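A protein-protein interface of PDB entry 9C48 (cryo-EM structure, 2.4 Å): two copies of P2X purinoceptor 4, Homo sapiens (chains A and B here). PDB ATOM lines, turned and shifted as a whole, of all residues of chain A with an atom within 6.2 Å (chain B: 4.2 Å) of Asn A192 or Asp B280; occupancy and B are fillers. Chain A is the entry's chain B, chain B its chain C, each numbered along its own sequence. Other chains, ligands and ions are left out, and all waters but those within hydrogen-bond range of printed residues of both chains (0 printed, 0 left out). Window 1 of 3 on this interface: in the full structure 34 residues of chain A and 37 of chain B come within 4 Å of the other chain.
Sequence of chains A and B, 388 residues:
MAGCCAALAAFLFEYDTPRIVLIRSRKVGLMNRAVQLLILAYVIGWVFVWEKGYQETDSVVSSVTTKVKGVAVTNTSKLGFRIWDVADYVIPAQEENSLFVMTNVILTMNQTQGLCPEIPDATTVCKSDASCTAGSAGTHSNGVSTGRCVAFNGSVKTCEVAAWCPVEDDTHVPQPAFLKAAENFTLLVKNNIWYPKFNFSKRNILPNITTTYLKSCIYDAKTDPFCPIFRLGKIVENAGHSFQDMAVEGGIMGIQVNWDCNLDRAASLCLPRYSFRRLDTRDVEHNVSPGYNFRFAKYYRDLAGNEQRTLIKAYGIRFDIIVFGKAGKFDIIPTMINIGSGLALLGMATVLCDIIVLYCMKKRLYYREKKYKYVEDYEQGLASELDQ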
ATOM      1  N   VAL A  61     -18.561  12.356  -5.109  1.00  0.00           N
ATOM      2  CA  VAL A  61     -19.999  12.583  -5.019  1.00  0.00           C
ATOM      3  C   VAL A  61     -20.334  13.662  -6.036  1.00  0.00           C
ATOM      4  O   VAL A  61     -19.800  14.776  -5.960  1.00  0.00           O
ATOM      5  CB  VAL A  61     -20.427  13.003  -3.603  1.00  0.00           C
ATOM      6  CG1 VAL A  61     -21.910  13.327  -3.567  1.00  0.00           C
ATOM      7  CG2 VAL A  61     -20.090  11.916  -2.601  1.00  0.00           C
ATOM      8  N   SER A  62     -21.206  13.343  -6.987  1.00  0.00           N
ATOM      9  CA  SER A  62     -21.454  14.213  -8.124  1.00  0.00           C
ATOM     10  C   SER A  62     -22.926  14.585  -8.223  1.00  0.00           C
ATOM     11  O   SER A  62     -23.808  13.786  -7.898  1.00  0.00           O
ATOM     12  CB  SER A  62     -21.009  13.552  -9.432  1.00  0.00           C
ATOM     13  OG  SER A  62     -21.770  12.392  -9.703  1.00  0.00           O
ATOM     14  N   SER A  63     -23.149  15.815  -8.695  1.00  0.00           N
ATOM     15  CA  SER A  63     -24.514  16.304  -8.986  1.00  0.00           C
ATOM     16  C   SER A  63     -24.490  16.764 -10.448  1.00  0.00           C
ATOM     17  O   SER A  63     -23.539  17.474 -10.808  1.00  0.00           O
ATOM     18  CB  SER A  63     -24.931  17.405  -8.043  1.00  0.00           C
ATOM     19  OG  SER A  63     -24.114  18.554  -8.197  1.00  0.00           O
ATOM     20  N   VAL A  64     -25.474  16.372 -11.256  1.00  0.00           N
ATOM     21  CA  VAL A  64     -25.526  16.676 -12.680  1.00  0.00           C
ATOM     22  C   VAL A  64     -26.835  17.385 -12.990  1.00  0.00           C
ATOM     23  O   VAL A  64     -27.908  16.922 -12.589  1.00  0.00           O
ATOM     24  CB  VAL A  64     -25.383  15.404 -13.538  1.00  0.00           C
ATOM     25  CG1 VAL A  64     -25.680  15.708 -14.992  1.00  0.00           C
ATOM     26  CG2 VAL A  64     -23.991  14.826 -13.395  1.00  0.00           C
ATOM     27  N   THR A  65     -26.746  18.507 -13.700  1.00  0.00           N
ATOM     28  CA  THR A  65     -27.905  19.224 -14.209  1.00  0.00           C
ATOM     29  C   THR A  65     -27.701  19.497 -15.691  1.00  0.00           C
ATOM     30  O   THR A  65     -26.577  19.722 -16.145  1.00  0.00           O
ATOM     31  CB  THR A  65     -28.136  20.543 -13.459  1.00  0.00           C
ATOM     32  OG1 THR A  65     -26.878  21.167 -13.182  1.00  0.00           O
ATOM     33  CG2 THR A  65     -28.847  20.283 -12.149  1.00  0.00           C
ATOM     34  N   LYS A 190     -23.842  20.440 -16.555  1.00  0.00           N
ATOM     35  CA  LYS A 190     -23.227  21.059 -15.385  1.00  0.00           C
ATOM     36  C   LYS A 190     -23.004  19.971 -14.344  1.00  0.00           C
ATOM     37  O   LYS A 190     -23.961  19.402 -13.816  1.00  0.00           O
ATOM     38  CB  LYS A 190     -24.103  22.178 -14.828  1.00  0.00           C
ATOM     39  CG  LYS A 190     -24.242  23.373 -15.746  1.00  0.00           C
ATOM     40  CD  LYS A 190     -25.251  24.373 -15.210  1.00  0.00           C
ATOM     41  CE  LYS A 190     -24.914  24.804 -13.796  1.00  0.00           C
ATOM     42  NZ  LYS A 190     -25.882  25.818 -13.299  1.00  0.00           N
ATOM     43  N   ASN A 191     -21.741  19.688 -14.046  1.00  0.00           N
ATOM     44  CA  ASN A 191     -21.368  18.620 -13.130  1.00  0.00           C
ATOM     45  C   ASN A 191     -20.625  19.221 -11.947  1.00  0.00           C
ATOM     46  O   ASN A 191     -19.583  19.856 -12.126  1.00  0.00           O
ATOM     47  CB  ASN A 191     -20.505  17.575 -13.837  1.00  0.00           C
ATOM     48  CG  ASN A 191     -20.214  16.372 -12.973  1.00  0.00           C
ATOM     49  OD1 ASN A 191     -20.958  16.060 -12.046  1.00  0.00           O
ATOM     50  ND2 ASN A 191     -19.122  15.691 -13.266  1.00  0.00           N
ATOM     51  N   ASN A 192     -21.161  19.022 -10.749  1.00  0.00           N
ATOM     52  CA  ASN A 192     -20.531  19.468  -9.515  1.00  0.00           C
ATOM     53  C   ASN A 192     -20.031  18.241  -8.767  1.00  0.00           C
ATOM     54  O   ASN A 192     -20.819  17.349  -8.444  1.00  0.00           O
ATOM     55  CB  ASN A 192     -21.519  20.255  -8.651  1.00  0.00           C
ATOM     56  CG  ASN A 192     -21.627  21.706  -9.062  1.00  0.00           C
ATOM     57  OD1 ASN A 192     -20.718  22.496  -8.830  1.00  0.00           O
ATOM     58  ND2 ASN A 192     -22.748  22.064  -9.672  1.00  0.00           N
ATOM     59  N   ILE A 193     -18.731  18.195  -8.490  1.00  0.00           N
ATOM     60  CA  ILE A 193     -18.115  17.047  -7.836  1.00  0.00           C
ATOM     61  C   ILE A 193     -17.602  17.471  -6.470  1.00  0.00           C
ATOM     62  O   ILE A 193     -17.199  18.622  -6.273  1.00  0.00           O
ATOM     63  CB  ILE A 193     -16.978  16.438  -8.684  1.00  0.00           C
ATOM     64  CG1 ILE A 193     -15.892  17.476  -8.972  1.00  0.00           C
ATOM     65  CG2 ILE A 193     -17.532  15.845  -9.966  1.00  0.00           C
ATOM     66  CD1 ILE A 193     -14.504  16.900  -9.021  1.00  0.00           C
ATOM     67  N   TRP A 194     -17.621  16.536  -5.525  1.00  0.00           N
ATOM     68  CA  TRP A 194     -17.191  16.799  -4.159  1.00  0.00           C
ATOM     69  C   TRP A 194     -16.488  15.567  -3.615  1.00  0.00           C
ATOM     70  O   TRP A 194     -17.001  14.453  -3.738  1.00  0.00           O
ATOM     71  CB  TRP A 194     -18.388  17.177  -3.276  1.00  0.00           C
ATOM     72  CG  TRP A 194     -18.108  17.212  -1.806  1.00  0.00           C
ATOM     73  CD1 TRP A 194     -17.029  17.771  -1.191  1.00  0.00           C
ATOM     74  CD2 TRP A 194     -18.941  16.695  -0.763  1.00  0.00           C
ATOM     75  NE1 TRP A 194     -17.128  17.617   0.170  1.00  0.00           N
ATOM     76  CE2 TRP A 194     -18.294  16.961   0.459  1.00  0.00           C
ATOM     77  CE3 TRP A 194     -20.170  16.027  -0.743  1.00  0.00           C
ATOM     78  CZ2 TRP A 194     -18.833  16.584   1.686  1.00  0.00           C
ATOM     79  CZ3 TRP A 194     -20.703  15.652   0.476  1.00  0.00           C
ATOM     80  CH2 TRP A 194     -20.035  15.931   1.673  1.00  0.00           C
ATOM     81  N   LYS A 202     -15.443  21.236  -6.958  1.00  0.00           N
ATOM     82  CA  LYS A 202     -15.337  22.069  -8.150  1.00  0.00           C
ATOM     83  C   LYS A 202     -16.374  21.591  -9.159  1.00  0.00           C
ATOM     84  O   LYS A 202     -17.081  20.608  -8.933  1.00  0.00           O
ATOM     85  CB  LYS A 202     -13.918  22.036  -8.725  1.00  0.00           C
ATOM     86  CG  LYS A 202     -13.566  20.781  -9.487  1.00  0.00           C
ATOM     87  CD  LYS A 202     -12.204  20.912 -10.141  1.00  0.00           C
ATOM     88  CE  LYS A 202     -12.079  22.209 -10.914  1.00  0.00           C
ATOM     89  NZ  LYS A 202     -10.697  22.432 -11.410  1.00  0.00           N
ATOM     90  N   ARG A 203     -16.479  22.323 -10.262  1.00  0.00           N
ATOM     91  CA  ARG A 203     -17.426  21.958 -11.305  1.00  0.00           C
ATOM     92  C   ARG A 203     -16.724  21.830 -12.642  1.00  0.00           C
ATOM     93  O   ARG A 203     -15.581  22.250 -12.789  1.00  0.00           O
ATOM     94  CB  ARG A 203     -18.569  22.974 -11.394  1.00  0.00           C
ATOM     95  CG  ARG A 203     -18.149  24.410 -11.637  1.00  0.00           C
ATOM     96  CD  ARG A 203     -19.378  25.277 -11.847  1.00  0.00           C
ATOM     97  NE  ARG A 203     -19.040  26.662 -12.149  1.00  0.00           N
ATOM     98  CZ  ARG A 203     -19.930  27.593 -12.473  1.00  0.00           C
ATOM     99  NH1 ARG A 203     -21.218  27.286 -12.542  1.00  0.00           N
ATOM    100  NH2 ARG A 203     -19.532  28.829 -12.733  1.00  0.00           N
ATOM    101  N   ASN A 204     -17.407  21.253 -13.616  1.00  0.00           N
ATOM    102  CA  ASN A 204     -16.814  21.036 -14.931  1.00  0.00           C
ATOM    103  C   ASN A 204     -16.774  22.309 -15.766  1.00  0.00           C
ATOM    104  O   ASN A 204     -16.101  22.334 -16.799  1.00  0.00           O
ATOM    105  CB  ASN A 204     -17.568  19.932 -15.677  1.00  0.00           C
ATOM    106  CG  ASN A 204     -18.952  20.357 -16.108  1.00  0.00           C
ATOM    107  OD1 ASN A 204     -19.604  21.158 -15.447  1.00  0.00           O
ATOM    108  ND2 ASN A 204     -19.411  19.814 -17.227  1.00  0.00           N
ATOM    109  N   GLY B 251     -30.411  26.723  -6.299  1.00  0.00           N
ATOM    110  CA  GLY B 251     -29.180  26.010  -6.039  1.00  0.00           C
ATOM    111  C   GLY B 251     -29.456  24.546  -5.770  1.00  0.00           C
ATOM    112  O   GLY B 251     -30.562  24.054  -5.988  1.00  0.00           O
ATOM    113  N   ILE B 252     -28.419  23.858  -5.300  1.00  0.00           N
ATOM    114  CA  ILE B 252     -28.488  22.443  -4.947  1.00  0.00           C
ATOM    115  C   ILE B 252     -28.065  22.302  -3.493  1.00  0.00           C
ATOM    116  O   ILE B 252     -27.028  22.839  -3.090  1.00  0.00           O
ATOM    117  CB  ILE B 252     -27.592  21.576  -5.852  1.00  0.00           C
ATOM    118  CG1 ILE B 252     -27.716  21.986  -7.322  1.00  0.00           C
ATOM    119  CG2 ILE B 252     -27.939  20.108  -5.684  1.00  0.00           C
ATOM    120  CD1 ILE B 252     -29.040  21.647  -7.942  1.00  0.00           C
ATOM    121  N   ARG B 278     -24.136  22.527   0.891  1.00  0.00           N
ATOM    122  CA  ARG B 278     -24.487  23.068  -0.414  1.00  0.00           C
ATOM    123  C   ARG B 278     -23.623  22.429  -1.495  1.00  0.00           C
ATOM    124  O   ARG B 278     -22.397  22.375  -1.372  1.00  0.00           O
ATOM    125  CB  ARG B 278     -24.317  24.584  -0.421  1.00  0.00           C
ATOM    126  CG  ARG B 278     -24.697  25.223  -1.735  1.00  0.00           C
ATOM    127  CD  ARG B 278     -24.855  26.719  -1.618  1.00  0.00           C
ATOM    128  NE  ARG B 278     -25.387  27.290  -2.850  1.00  0.00           N
ATOM    129  CZ  ARG B 278     -25.706  28.564  -3.011  1.00  0.00           C
ATOM    130  NH1 ARG B 278     -25.557  29.442  -2.033  1.00  0.00           N
ATOM    131  NH2 ARG B 278     -26.188  28.970  -4.181  1.00  0.00           N
ATOM    132  N   LEU B 279     -24.263  21.956  -2.565  1.00  0.00           N
ATOM    133  CA  LEU B 279     -23.581  21.147  -3.566  1.00  0.00           C
ATOM    134  C   LEU B 279     -23.179  21.912  -4.819  1.00  0.00           C
ATOM    135  O   LEU B 279     -22.255  21.475  -5.513  1.00  0.00           O
ATOM    136  CB  LEU B 279     -24.460  19.959  -3.978  1.00  0.00           C
ATOM    137  CG  LEU B 279     -24.764  18.908  -2.912  1.00  0.00           C
ATOM    138  CD1 LEU B 279     -25.543  17.760  -3.516  1.00  0.00           C
ATOM    139  CD2 LEU B 279     -23.490  18.408  -2.261  1.00  0.00           C
ATOM    140  N   ASP B 280     -23.835  23.025  -5.137  1.00  0.00           N
ATOM    141  CA  ASP B 280     -23.537  23.758  -6.360  1.00  0.00           C
ATOM    142  C   ASP B 280     -22.432  24.775  -6.094  1.00  0.00           C
ATOM    143  O   ASP B 280     -22.526  25.581  -5.162  1.00  0.00           O
ATOM    144  CB  ASP B 280     -24.790  24.434  -6.920  1.00  0.00           C
ATOM    145  CG  ASP B 280     -25.371  25.474  -5.987  1.00  0.00           C
ATOM    146  OD1 ASP B 280     -25.446  25.211  -4.772  1.00  0.00           O
ATOM    147  OD2 ASP B 280     -25.755  26.559  -6.470  1.00  0.00           O
ATOM    148  N   THR B 281     -21.376  24.717  -6.899  1.00  0.00           N
ATOM    149  CA  THR B 281     -20.259  25.640  -6.758  1.00  0.00           C
ATOM    150  C   THR B 281     -20.585  26.973  -7.417  1.00  0.00           C
ATOM    151  O   THR B 281     -21.072  27.022  -8.550  1.00  0.00           O
ATOM    152  CB  THR B 281     -18.995  25.040  -7.377  1.00  0.00           C
ATOM    153  OG1 THR B 281     -18.812  23.705  -6.888  1.00  0.00           O
ATOM    154  CG2 THR B 281     -17.777  25.872  -7.025  1.00  0.00           C
ATOM    155  N   ARG B 282     -20.314  28.057  -6.701  1.00  0.00           N
ATOM    156  CA  ARG B 282     -20.658  29.402  -7.138  1.00  0.00           C
ATOM    157  C   ARG B 282     -19.414  30.112  -7.649  1.00  0.00           C
ATOM    158  O   ARG B 282     -18.336  29.994  -7.057  1.00  0.00           O
ATOM    159  CB  ARG B 282     -21.289  30.202  -5.996  1.00  0.00           C
ATOM    160  CG  ARG B 282     -22.178  29.378  -5.079  1.00  0.00           C
ATOM    161  CD  ARG B 282     -22.252  29.992  -3.694  1.00  0.00           C
ATOM    162  NE  ARG B 282     -22.745  31.363  -3.726  1.00  0.00           N
ATOM    163  CZ  ARG B 282     -22.692  32.199  -2.700  1.00  0.00           C
ATOM    164  NH1 ARG B 282     -22.152  31.844  -1.546  1.00  0.00           N
ATOM    165  NH2 ARG B 282     -23.189  33.425  -2.837  1.00  0.00           N
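The side-chain amide oxygen (OD1) of Asn A192 lies within hydrogen-bond range of the side-chain hydroxyl (OG1) of Thr B281, 3.0 Å away.
N of Ser A63 is in hydrogen-bond range of O of Asn A192 (2.8 Å).
N of Ile A193 is in hydrogen-bond range of O of Lys A202, 3.0 Å away.
O of Ile B252 is in hydrogen-bond range of N of Leu B279 (2.9 Å).
The side-chain carboxylate (OD1) of Asp B280 is in hydrogen-bond range of the backbone NH (N) of Ile B252, 3.3 Å away.
NE of Arg B278 is in salt-bridge range of OD1 of Asp B280 (2.8 Å).
O of Leu B279 touches CB of Asn A192 (3.4 Å).
Asn A192 touches Asp B280.
C of Lys A202 touches OG1 of Thr B281 (3.9 Å).
Val A64 touches none of the printed residues of chain B.
Of the printed residues of chain B, Asn A192 touches Leu B279 (3.4 Å), Asp B280 (3.8 Å) and Thr B281 (3.0 Å).
Of the printed residues of chain B, Lys A202 touches Thr B281 (3.9 Å).
Of the printed residues of chain A, Leu B279 touches Asn A192.
Of the printed residues of chain A, Asp B280 touches Asn A192.
Printed residues of chain A within 4 Å of Thr B281: Asn A192 and Lys A202.
The nearest printed residue of chain A that does not touch Leu B279 is Trp A194 (4.4 Å).
Among the printed residues, 4 pairs touch across the chains.
Among the printed residues, no Asp or Glu carboxylate lies within 4 Å of a Lys or Arg side-chain nitrogen of the other chain.
No position is printed for both chains.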
